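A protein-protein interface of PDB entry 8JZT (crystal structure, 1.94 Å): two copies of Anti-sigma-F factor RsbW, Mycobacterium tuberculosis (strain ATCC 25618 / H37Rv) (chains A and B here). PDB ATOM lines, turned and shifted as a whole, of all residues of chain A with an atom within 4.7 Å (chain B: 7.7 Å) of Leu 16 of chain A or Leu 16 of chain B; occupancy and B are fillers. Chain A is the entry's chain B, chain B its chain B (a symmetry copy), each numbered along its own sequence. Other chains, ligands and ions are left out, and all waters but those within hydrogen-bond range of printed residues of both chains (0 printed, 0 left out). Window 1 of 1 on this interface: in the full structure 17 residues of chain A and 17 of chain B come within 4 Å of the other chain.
Of the 11 printed residues of chain A, 7 touch a printed residue of chain B.
Printed residues of chain A that touch a printed residue of chain B: Val 14, Glu 15, Leu 16, Asn 17, Val 18, Leu 31 and Ile 35.
Hydrophobic or aromatic side chains of chain A within 4 Å of the printed part of chain B: Val 14, Leu 16, Val 18, Leu 31 and Ile 35.
Along chain A the printed residues that touch a printed residue of chain B span positions 14 to 35.
Printed residues of chain B that touch a printed residue of chain A: Ala 13, Val 14, Glu 15, Leu 16, Asn 17, Val 18, Leu 31 and Ile 35.
Among the printed residues, no Asp or Glu carboxylate lies within 4 Å of a Lys or Arg side-chain nitrogen of the other chain.
Val 14 of chain A touches Asn 17 of chain B, and with the chains exchanged Asn 17 of chain A touches Val 14 of chain B.
Val 14 of chain A touches Val 18 of chain B, and with the chains exchanged Val 18 of chain A touches Val 14 of chain B.
Glu 15 of chain A touches its own counterpart, Glu 15 of chain B.
Glu 15 of chain A touches Leu 16 of chain B, and with the chains exchanged Leu 16 of chain A touches Glu 15 of chain B.
Of the 15 pairs that touch across the chains among the printed residues, 13 have their exchanged pair printed and touching as well.
Of chain B, only Glu 15 (3.3 Å) and Leu 16 (3.2 Å) come within 4 Å of Leu 16 of chain A.
Printed residues of chain A within 4 Å of Glu 15 of chain B: Glu 15 (3.6 Å), Leu 16 (3.3 Å) and Asn 17 (2.9 Å).
Of chain A, only Glu 15 (3.3 Å) and Leu 16 (3.2 Å) come within 4 Å of Leu 16 of chain B.
Of the printed residues of chain A, Asn 17 of chain B touches Val 14 (3.4 Å), Glu 15 (2.9 Å) and Asn 17 (3.6 Å).
Val 74 of chain B touches none of the printed residues of chain A.
The nearest residue of chain B that does not touch Leu 16 of chain A is Val 14 of chain B (4.7 Å).
The nearest printed residue of chain B that does not touch Leu 31 of chain A is Leu 31 of chain B (4.1 Å).
The backbone carbonyl oxygen of Glu 15 of chain A is in hydrogen-bond range of the backbone NH of Asn 17 of chain B (2.9 Å).
The backbone NH of Asn 17 of chain A sits at hydrogen-bond distance from the backbone carbonyl oxygen of Glu 15 of chain B (2.9 Å).
NH1 of Arg 71 of chain A is in salt-bridge range of OE2 of Glu 15 of chain A (2.9 Å).
The backbone NH (N) of Val 14 of chain B is in hydrogen-bond range of the backbone carbonyl oxygen (O) of Val 74 of chain B (2.9 Å).
ND2 of Asn 17 of chain B lies within hydrogen-bond range of OE2 of Glu 15 of chain B, 2.9 Å away.
The side-chain carboxylate (OE2) of Glu 15 of chain B is in salt-bridge range of the guanidinium group (NH1) of Arg 71 of chain B (2.9 Å).
N of Leu 16 of chain B lies within hydrogen-bond range of O of Leu 72 of chain B.
The backbone NH (N) of Leu 70 of chain B is in hydrogen-bond range of the backbone carbonyl oxygen (O) of Val 18 of chain B (2.8 Å).
Among the printed residues, merely in contact across the chains: Val 14 of chain A with Asn 17 of chain B, Val 14 of chain A with Val 18 of chain B, Glu 15 of chain A with Glu 15 of chain B, Glu 15 of chain A with Leu 16 of chain B, Leu 16 of chain A with Glu 15 of chain B, Leu 16 of chain A with Leu 16 of chain B, Asn 17 of chain A with Ala 13 of chain B, Asn 17 of chain A with Val 14 of chain B, Asn 17 of chain A with Asn 17 of chain B, Val 18 of chain A with Ala 13 of chain B, Val 18 of chain A with Val 14 of chain B, Leu 31 of chain A with Ile 35 of chain B and Ile 35 of chain A with Leu 31 of chain B.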
ATOM      1  N   VAL A  14       4.038 -19.632 -24.759  1.00  0.00           N
ATOM      2  CA  VAL A  14       5.442 -19.704 -25.149  1.00  0.00           C
ATOM      3  C   VAL A  14       5.552 -20.530 -26.419  1.00  0.00           C
ATOM      4  O   VAL A  14       4.972 -21.619 -26.523  1.00  0.00           O
ATOM      5  CB  VAL A  14       6.355 -20.269 -24.036  1.00  0.00           C
ATOM      6  CG1 VAL A  14       5.793 -21.488 -23.441  1.00  0.00           C
ATOM      7  CG2 VAL A  14       7.782 -20.510 -24.552  1.00  0.00           C
ATOM      8  N   GLU A  15       6.272 -19.993 -27.391  1.00  0.00           N
ATOM      9  CA  GLU A  15       6.576 -20.705 -28.624  1.00  0.00           C
ATOM     10  C   GLU A  15       7.991 -21.243 -28.515  1.00  0.00           C
ATOM     11  O   GLU A  15       8.903 -20.509 -28.128  1.00  0.00           O
ATOM     12  CB  GLU A  15       6.453 -19.772 -29.828  1.00  0.00           C
ATOM     13  CG  GLU A  15       6.656 -20.461 -31.189  1.00  0.00           C
ATOM     14  CD  GLU A  15       6.736 -19.427 -32.297  1.00  0.00           C
ATOM     15  OE1 GLU A  15       5.786 -18.623 -32.419  1.00  0.00           O
ATOM     16  OE2 GLU A  15       7.768 -19.378 -32.994  1.00  0.00           O
ATOM     17  N   LEU A  16       8.170 -22.524 -28.817  1.00  0.00           N
ATOM     18  CA  LEU A  16       9.493 -23.139 -28.836  1.00  0.00           C
ATOM     19  C   LEU A  16       9.788 -23.566 -30.262  1.00  0.00           C
ATOM     20  O   LEU A  16       8.909 -24.118 -30.931  1.00  0.00           O
ATOM     21  CB  LEU A  16       9.547 -24.385 -27.948  1.00  0.00           C
ATOM     22  CG  LEU A  16       8.970 -24.338 -26.528  1.00  0.00           C
ATOM     23  CD1 LEU A  16       8.980 -25.720 -25.907  1.00  0.00           C
ATOM     24  CD2 LEU A  16       9.740 -23.434 -25.703  1.00  0.00           C
ATOM     25  N   ASN A  17      11.021 -23.360 -30.723  1.00  0.00           N
ATOM     26  CA  ASN A  17      11.432 -23.875 -32.027  1.00  0.00           C
ATOM     27  C   ASN A  17      12.754 -24.614 -31.904  1.00  0.00           C
ATOM     28  O   ASN A  17      13.711 -24.058 -31.373  1.00  0.00           O
ATOM     29  CB  ASN A  17      11.599 -22.754 -33.051  1.00  0.00           C
ATOM     30  CG  ASN A  17      10.326 -21.994 -33.264  1.00  0.00           C
ATOM     31  OD1 ASN A  17       9.517 -22.382 -34.085  1.00  0.00           O
ATOM     32  ND2 ASN A  17      10.140 -20.911 -32.529  1.00  0.00           N
ATOM     33  N   VAL A  18      12.812 -25.839 -32.426  1.00  0.00           N
ATOM     34  CA  VAL A  18      14.044 -26.622 -32.468  1.00  0.00           C
ATOM     35  C   VAL A  18      14.110 -27.292 -33.833  1.00  0.00           C
ATOM     36  O   VAL A  18      13.087 -27.470 -34.509  1.00  0.00           O
ATOM     37  CB  VAL A  18      14.112 -27.709 -31.360  1.00  0.00           C
ATOM     38  CG1 VAL A  18      13.994 -27.105 -29.972  1.00  0.00           C
ATOM     39  CG2 VAL A  18      13.023 -28.760 -31.579  1.00  0.00           C
ATOM     40  N   LEU A  28      12.701 -31.396 -25.876  1.00  0.00           N
ATOM     41  CA  LEU A  28      11.292 -30.994 -25.935  1.00  0.00           C
ATOM     42  C   LEU A  28      10.492 -31.546 -24.750  1.00  0.00           C
ATOM     43  O   LEU A  28       9.673 -30.835 -24.163  1.00  0.00           O
ATOM     44  CB  LEU A  28      10.672 -31.453 -27.261  1.00  0.00           C
ATOM     45  CG  LEU A  28      11.100 -30.621 -28.486  1.00  0.00           C
ATOM     46  CD1 LEU A  28      10.566 -31.245 -29.792  1.00  0.00           C
ATOM     47  CD2 LEU A  28      10.647 -29.144 -28.383  1.00  0.00           C
ATOM     48  N   LEU A  31      11.373 -29.403 -21.651  1.00  0.00           N
ATOM     49  CA  LEU A  31      10.825 -28.046 -21.631  1.00  0.00           C
ATOM     50  C   LEU A  31       9.311 -28.062 -21.439  1.00  0.00           C
ATOM     51  O   LEU A  31       8.767 -27.208 -20.737  1.00  0.00           O
ATOM     52  CB  LEU A  31      11.183 -27.321 -22.927  1.00  0.00           C
ATOM     53  CG  LEU A  31      12.674 -27.143 -23.176  1.00  0.00           C
ATOM     54  CD1 LEU A  31      12.823 -26.426 -24.479  1.00  0.00           C
ATOM     55  CD2 LEU A  31      13.271 -26.322 -22.025  1.00  0.00           C
ATOM     56  N   ILE A  35       7.216 -26.352 -18.332  1.00  0.00           N
ATOM     57  CA  ILE A  35       6.095 -25.421 -18.474  1.00  0.00           C
ATOM     58  C   ILE A  35       4.866 -25.914 -17.702  1.00  0.00           C
ATOM     59  O   ILE A  35       4.138 -25.117 -17.103  1.00  0.00           O
ATOM     60  CB  ILE A  35       5.737 -25.210 -19.955  1.00  0.00           C
ATOM     61  CG1 ILE A  35       6.896 -24.622 -20.755  1.00  0.00           C
ATOM     62  CG2 ILE A  35       4.461 -24.331 -20.099  1.00  0.00           C
ATOM     63  CD1 ILE A  35       6.725 -24.853 -22.259  1.00  0.00           C
ATOM     64  N   LEU A  70      10.718 -27.924 -35.924  1.00  0.00           N
ATOM     65  CA  LEU A  70       9.574 -28.285 -35.096  1.00  0.00           C
ATOM     66  C   LEU A  70       9.178 -27.030 -34.326  1.00  0.00           C
ATOM     67  O   LEU A  70       9.971 -26.521 -33.529  1.00  0.00           O
ATOM     68  CB  LEU A  70       9.946 -29.418 -34.130  1.00  0.00           C
ATOM     69  CG  LEU A  70       8.840 -30.200 -33.372  1.00  0.00           C
ATOM     70  CD1 LEU A  70       8.276 -29.354 -32.246  1.00  0.00           C
ATOM     71  CD2 LEU A  70       7.694 -30.746 -34.257  1.00  0.00           C
ATOM     72  N   ARG A  71       7.958 -26.547 -34.545  1.00  0.00           N
ATOM     73  CA  ARG A  71       7.451 -25.334 -33.908  1.00  0.00           C
ATOM     74  C   ARG A  71       6.363 -25.725 -32.918  1.00  0.00           C
ATOM     75  O   ARG A  71       5.320 -26.247 -33.327  1.00  0.00           O
ATOM     76  CB  ARG A  71       6.893 -24.357 -34.948  1.00  0.00           C
ATOM     77  CG  ARG A  71       6.211 -23.146 -34.311  1.00  0.00           C
ATOM     78  CD  ARG A  71       5.506 -22.223 -35.314  1.00  0.00           C
ATOM     79  NE  ARG A  71       6.298 -21.882 -36.494  1.00  0.00           N
ATOM     80  CZ  ARG A  71       6.952 -20.739 -36.663  1.00  0.00           C
ATOM     81  NH1 ARG A  71       6.997 -19.817 -35.715  1.00  0.00           N
ATOM     82  NH2 ARG A  71       7.565 -20.509 -37.821  1.00  0.00           N
ATOM     83  N   LEU A  72       6.593 -25.457 -31.628  1.00  0.00           N
ATOM     84  CA  LEU A  72       5.709 -25.904 -30.556  1.00  0.00           C
ATOM     85  C   LEU A  72       5.218 -24.683 -29.790  1.00  0.00           C
ATOM     86  O   LEU A  72       6.037 -23.909 -29.285  1.00  0.00           O
ATOM     87  CB  LEU A  72       6.467 -26.875 -29.631  1.00  0.00           C
ATOM     88  CG  LEU A  72       5.711 -27.524 -28.475  1.00  0.00           C
ATOM     89  CD1 LEU A  72       4.631 -28.428 -29.004  1.00  0.00           C
ATOM     90  CD2 LEU A  72       6.673 -28.350 -27.642  1.00  0.00           C
ATOM     91  N   ALA B  13      20.068 -26.021 -30.938  1.00  0.00           N
ATOM     92  CA  ALA B  13      19.606 -24.716 -30.482  1.00  0.00           C
ATOM     93  C   ALA B  13      18.108 -24.750 -30.217  1.00  0.00           C
ATOM     94  O   ALA B  13      17.372 -25.529 -30.827  1.00  0.00           O
ATOM     95  CB  ALA B  13      19.913 -23.647 -31.533  1.00  0.00           C
ATOM     96  N   VAL B  14      17.648 -23.900 -29.301  1.00  0.00           N
ATOM     97  CA  VAL B  14      16.214 -23.734 -29.089  1.00  0.00           C
ATOM     98  C   VAL B  14      15.896 -22.249 -29.063  1.00  0.00           C
ATOM     99  O   VAL B  14      16.572 -21.463 -28.385  1.00  0.00           O
ATOM    100  CB  VAL B  14      15.702 -24.436 -27.810  1.00  0.00           C
ATOM    101  CG1 VAL B  14      16.558 -24.144 -26.653  1.00  0.00           C
ATOM    102  CG2 VAL B  14      14.237 -24.074 -27.521  1.00  0.00           C
ATOM    103  N   GLU B  15      14.885 -21.866 -29.827  1.00  0.00           N
ATOM    104  CA  GLU B  15      14.374 -20.503 -29.824  1.00  0.00           C
ATOM    105  C   GLU B  15      13.121 -20.476 -28.968  1.00  0.00           C
ATOM    106  O   GLU B  15      12.248 -21.332 -29.125  1.00  0.00           O
ATOM    107  CB  GLU B  15      14.057 -20.045 -31.247  1.00  0.00           C
ATOM    108  CG  GLU B  15      13.607 -18.577 -31.356  1.00  0.00           C
ATOM    109  CD  GLU B  15      13.107 -18.282 -32.758  1.00  0.00           C
ATOM    110  OE1 GLU B  15      13.876 -18.514 -33.716  1.00  0.00           O
ATOM    111  OE2 GLU B  15      11.934 -17.885 -32.902  1.00  0.00           O
ATOM    112  N   LEU B  16      13.046 -19.524 -28.045  1.00  0.00           N
ATOM    113  CA  LEU B  16      11.859 -19.336 -27.218  1.00  0.00           C
ATOM    114  C   LEU B  16      11.269 -17.978 -27.551  1.00  0.00           C
ATOM    115  O   LEU B  16      12.014 -17.002 -27.682  1.00  0.00           O
ATOM    116  CB  LEU B  16      12.203 -19.351 -25.727  1.00  0.00           C
ATOM    117  CG  LEU B  16      13.113 -20.449 -25.163  1.00  0.00           C
ATOM    118  CD1 LEU B  16      13.450 -20.163 -23.713  1.00  0.00           C
ATOM    119  CD2 LEU B  16      12.465 -21.738 -25.261  1.00  0.00           C
ATOM    120  N   ASN B  17       9.943 -17.890 -27.646  1.00  0.00           N
ATOM    121  CA  ASN B  17       9.286 -16.596 -27.812  1.00  0.00           C
ATOM    122  C   ASN B  17       8.152 -16.453 -26.811  1.00  0.00           C
ATOM    123  O   ASN B  17       7.296 -17.330 -26.735  1.00  0.00           O
ATOM    124  CB  ASN B  17       8.711 -16.430 -29.218  1.00  0.00           C
ATOM    125  CG  ASN B  17       9.772 -16.520 -30.272  1.00  0.00           C
ATOM    126  OD1 ASN B  17      10.388 -15.523 -30.599  1.00  0.00           O
ATOM    127  ND2 ASN B  17       9.991 -17.708 -30.807  1.00  0.00           N
ATOM    128  N   VAL B  18       8.129 -15.338 -26.080  1.00  0.00           N
ATOM    129  CA  VAL B  18       7.045 -15.024 -25.152  1.00  0.00           C
ATOM    130  C   VAL B  18       6.723 -13.546 -25.314  1.00  0.00           C
ATOM    131  O   VAL B  18       7.553 -12.757 -25.790  1.00  0.00           O
ATOM    132  CB  VAL B  18       7.411 -15.309 -23.670  1.00  0.00           C
ATOM    133  CG1 VAL B  18       7.798 -16.762 -23.456  1.00  0.00           C
ATOM    134  CG2 VAL B  18       8.540 -14.384 -23.214  1.00  0.00           C
ATOM    135  N   LEU B  27       8.825 -17.416 -15.997  1.00  0.00           N
ATOM    136  CA  LEU B  27       8.815 -18.521 -16.953  1.00  0.00           C
ATOM    137  C   LEU B  27      10.134 -18.597 -17.717  1.00  0.00           C
ATOM    138  O   LEU B  27      10.696 -19.685 -17.888  1.00  0.00           O
ATOM    139  CB  LEU B  27       7.648 -18.353 -17.927  1.00  0.00           C
ATOM    140  CG  LEU B  27       7.644 -19.318 -19.126  1.00  0.00           C
ATOM    141  CD1 LEU B  27       7.417 -20.738 -18.597  1.00  0.00           C
ATOM    142  CD2 LEU B  27       6.574 -18.940 -20.179  1.00  0.00           C
ATOM    143  N   LEU B  28      10.666 -17.450 -18.149  1.00  0.00           N
ATOM    144  CA  LEU B  28      11.945 -17.441 -18.867  1.00  0.00           C
ATOM    145  C   LEU B  28      13.089 -17.976 -17.999  1.00  0.00           C
ATOM    146  O   LEU B  28      13.928 -18.747 -18.474  1.00  0.00           O
ATOM    147  CB  LEU B  28      12.262 -16.021 -19.355  1.00  0.00           C
ATOM    148  CG  LEU B  28      11.425 -15.563 -20.566  1.00  0.00           C
ATOM    149  CD1 LEU B  28      11.686 -14.077 -20.887  1.00  0.00           C
ATOM    150  CD2 LEU B  28      11.685 -16.429 -21.823  1.00  0.00           C
ATOM    151  N   ARG B  29      13.167 -17.561 -16.737  1.00  0.00           N
ATOM    152  CA  ARG B  29      14.207 -18.108 -15.864  1.00  0.00           C
ATOM    153  C   ARG B  29      14.077 -19.619 -15.732  1.00  0.00           C
ATOM    154  O   ARG B  29      15.081 -20.345 -15.719  1.00  0.00           O
ATOM    155  CB  ARG B  29      14.135 -17.473 -14.471  1.00  0.00           C
ATOM    156  CG  ARG B  29      14.681 -16.082 -14.373  1.00  0.00           C
ATOM    157  CD  ARG B  29      14.890 -15.694 -12.909  1.00  0.00           C
ATOM    158  NE  ARG B  29      13.609 -15.361 -12.323  1.00  0.00           N
ATOM    159  CZ  ARG B  29      12.924 -14.242 -12.534  1.00  0.00           C
ATOM    160  NH1 ARG B  29      13.427 -13.225 -13.231  1.00  0.00           N
ATOM    161  NH2 ARG B  29      11.695 -14.149 -12.049  1.00  0.00           N
ATOM    162  N   THR B  30      12.847 -20.117 -15.587  1.00  0.00           N
ATOM    163  CA  THR B  30      12.661 -21.561 -15.447  1.00  0.00           C
ATOM    164  C   THR B  30      13.148 -22.301 -16.687  1.00  0.00           C
ATOM    165  O   THR B  30      13.854 -23.313 -16.587  1.00  0.00           O
ATOM    166  CB  THR B  30      11.180 -21.860 -15.189  1.00  0.00           C
ATOM    167  OG1 THR B  30      10.783 -21.211 -13.981  1.00  0.00           O
ATOM    168  CG2 THR B  30      10.925 -23.364 -15.072  1.00  0.00           C
ATOM    169  N   LEU B  31      12.750 -21.828 -17.870  1.00  0.00           N
ATOM    170  CA  LEU B  31      13.096 -22.546 -19.099  1.00  0.00           C
ATOM    171  C   LEU B  31      14.596 -22.486 -19.372  1.00  0.00           C
ATOM    172  O   LEU B  31      15.180 -23.469 -19.832  1.00  0.00           O
ATOM    173  CB  LEU B  31      12.322 -21.959 -20.278  1.00  0.00           C
ATOM    174  CG  LEU B  31      10.807 -22.062 -20.172  1.00  0.00           C
ATOM    175  CD1 LEU B  31      10.234 -21.437 -21.403  1.00  0.00           C
ATOM    176  CD2 LEU B  31      10.419 -23.544 -20.075  1.00  0.00           C
ATOM    177  N   VAL B  32      15.232 -21.337 -19.100  1.00  0.00           N
ATOM    178  CA  VAL B  32      16.684 -21.216 -19.299  1.00  0.00           C
ATOM    179  C   VAL B  32      17.424 -22.166 -18.357  1.00  0.00           C
ATOM    180  O   VAL B  32      18.401 -22.826 -18.741  1.00  0.00           O
ATOM    181  CB  VAL B  32      17.130 -19.752 -19.096  1.00  0.00           C
ATOM    182  CG1 VAL B  32      18.653 -19.635 -18.917  1.00  0.00           C
ATOM    183  CG2 VAL B  32      16.623 -18.843 -20.234  1.00  0.00           C
ATOM    184  N   ILE B  35      17.164 -25.694 -19.651  1.00  0.00           N
ATOM    185  CA  ILE B  35      18.075 -25.959 -20.767  1.00  0.00           C
ATOM    186  C   ILE B  35      19.516 -26.136 -20.274  1.00  0.00           C
ATOM    187  O   ILE B  35      20.258 -26.977 -20.789  1.00  0.00           O
ATOM    188  CB  ILE B  35      18.009 -24.832 -21.812  1.00  0.00           C
ATOM    189  CG1 ILE B  35      16.616 -24.678 -22.414  1.00  0.00           C
ATOM    190  CG2 ILE B  35      19.074 -25.045 -22.926  1.00  0.00           C
ATOM    191  CD1 ILE B  35      16.425 -23.306 -23.065  1.00  0.00           C
ATOM    192  N   THR B  69       7.446  -8.903 -28.599  1.00  0.00           N
ATOM    193  CA  THR B  69       7.799 -10.286 -28.302  1.00  0.00           C
ATOM    194  C   THR B  69       9.256 -10.334 -27.866  1.00  0.00           C
ATOM    195  O   THR B  69      10.112  -9.718 -28.498  1.00  0.00           O
ATOM    196  CB  THR B  69       7.597 -11.171 -29.536  1.00  0.00           C
ATOM    197  OG1 THR B  69       6.215 -11.156 -29.907  1.00  0.00           O
ATOM    198  CG2 THR B  69       8.019 -12.591 -29.243  1.00  0.00           C
ATOM    199  N   LEU B  70       9.519 -11.031 -26.777  1.00  0.00           N
ATOM    200  CA  LEU B  70      10.876 -11.340 -26.340  1.00  0.00           C
ATOM    201  C   LEU B  70      11.281 -12.627 -27.050  1.00  0.00           C
ATOM    202  O   LEU B  70      10.658 -13.670 -26.838  1.00  0.00           O
ATOM    203  CB  LEU B  70      10.921 -11.525 -24.818  1.00  0.00           C
ATOM    204  CG  LEU B  70      12.280 -11.542 -24.067  1.00  0.00           C
ATOM    205  CD1 LEU B  70      12.993 -12.860 -24.301  1.00  0.00           C
ATOM    206  CD2 LEU B  70      13.224 -10.358 -24.386  1.00  0.00           C
ATOM    207  N   ARG B  71      12.327 -12.560 -27.870  1.00  0.00           N
ATOM    208  CA  ARG B  71      12.811 -13.700 -28.645  1.00  0.00           C
ATOM    209  C   ARG B  71      14.159 -14.130 -28.084  1.00  0.00           C
ATOM    210  O   ARG B  71      15.123 -13.359 -28.145  1.00  0.00           O
ATOM    211  CB  ARG B  71      12.946 -13.341 -30.128  1.00  0.00           C
ATOM    212  CG  ARG B  71      13.598 -14.456 -30.947  1.00  0.00           C
ATOM    213  CD  ARG B  71      13.890 -14.075 -32.405  1.00  0.00           C
ATOM    214  NE  ARG B  71      12.784 -13.422 -33.101  1.00  0.00           N
ATOM    215  CZ  ARG B  71      11.960 -14.027 -33.948  1.00  0.00           C
ATOM    216  NH1 ARG B  71      12.035 -15.328 -34.181  1.00  0.00           N
ATOM    217  NH2 ARG B  71      11.046 -13.305 -34.589  1.00  0.00           N
ATOM    218  N   LEU B  72      14.233 -15.359 -27.561  1.00  0.00           N
ATOM    219  CA  LEU B  72      15.415 -15.851 -26.858  1.00  0.00           C
ATOM    220  C   LEU B  72      15.915 -17.102 -27.568  1.00  0.00           C
ATOM    221  O   LEU B  72      15.155 -18.064 -27.718  1.00  0.00           O
ATOM    222  CB  LEU B  72      15.058 -16.148 -25.390  1.00  0.00           C
ATOM    223  CG  LEU B  72      16.166 -16.610 -24.447  1.00  0.00           C
ATOM    224  CD1 LEU B  72      17.186 -15.519 -24.272  1.00  0.00           C
ATOM    225  CD2 LEU B  72      15.571 -16.944 -23.092  1.00  0.00           C
ATOM    226  N   VAL B  73      17.180 -17.099 -28.006  1.00  0.00           N
ATOM    227  CA  VAL B  73      17.788 -18.275 -28.629  1.00  0.00           C
ATOM    228  C   VAL B  73      18.917 -18.760 -27.719  1.00  0.00           C
ATOM    229  O   VAL B  73      19.786 -17.971 -27.341  1.00  0.00           O
ATOM    230  CB  VAL B  73      18.320 -17.968 -30.044  1.00  0.00           C
ATOM    231  CG1 VAL B  73      18.856 -19.259 -30.718  1.00  0.00           C
ATOM    232  CG2 VAL B  73      17.221 -17.346 -30.913  1.00  0.00           C
ATOM    233  N   VAL B  74      18.885 -20.039 -27.346  1.00  0.00           N
ATOM    234  CA  VAL B  74      19.978 -20.696 -26.624  1.00  0.00           C
ATOM    235  C   VAL B  74      20.581 -21.716 -27.580  1.00  0.00           C
ATOM    236  O   VAL B  74      19.899 -22.649 -28.011  1.00  0.00           O
ATOM    237  CB  VAL B  74      19.505 -21.369 -25.327  1.00  0.00           C
ATOM    238  CG1 VAL B  74      20.685 -22.061 -24.596  1.00  0.00           C
ATOM    239  CG2 VAL B  74      18.792 -20.383 -24.443  1.00  0.00           C
ATOM    240  N   GLU B  84      21.104 -15.416 -27.348  1.00  0.00           N
ATOM    241  CA  GLU B  84      20.712 -14.180 -28.011  1.00  0.00           C
ATOM    242  C   GLU B  84      19.302 -13.799 -27.582  1.00  0.00           C
ATOM    243  O   GLU B  84      18.388 -14.620 -27.644  1.00  0.00           O
ATOM    244  CB  GLU B  84      20.805 -14.360 -29.522  1.00  0.00           C
ATOM    245  CG  GLU B  84      20.511 -13.129 -30.344  1.00  0.00           C
ATOM    246  CD  GLU B  84      21.079 -13.275 -31.749  1.00  0.00           C
ATOM    247  OE1 GLU B  84      22.325 -13.183 -31.926  1.00  0.00           O
ATOM    248  OE2 GLU B  84      20.276 -13.533 -32.658  1.00  0.00           O
ATOM    249  N   ALA B  85      19.115 -12.552 -27.151  1.00  0.00           N
ATOM    250  CA  ALA B  85      17.788 -12.104 -26.751  1.00  0.00           C
ATOM    251  C   ALA B  85      17.500 -10.766 -27.417  1.00  0.00           C
ATOM    252  O   ALA B  85      18.397  -9.927 -27.534  1.00  0.00           O
ATOM    253  CB  ALA B  85      17.666 -11.981 -25.241  1.00  0.00           C
ATOM    254  N   SER B  86      16.252 -10.562 -27.841  1.00  0.00           N
ATOM    255  CA  SER B  86      15.902  -9.327 -28.540  1.00  0.00           C
ATOM    256  C   SER B  86      14.406  -9.065 -28.406  1.00  0.00           C
ATOM    257  O   SER B  86      13.619  -9.980 -28.176  1.00  0.00           O
ATOM    258  CB  SER B  86      16.316  -9.394 -30.009  1.00  0.00           C
ATOM    259  OG  SER B  86      15.524 -10.333 -30.714  1.00  0.00           O
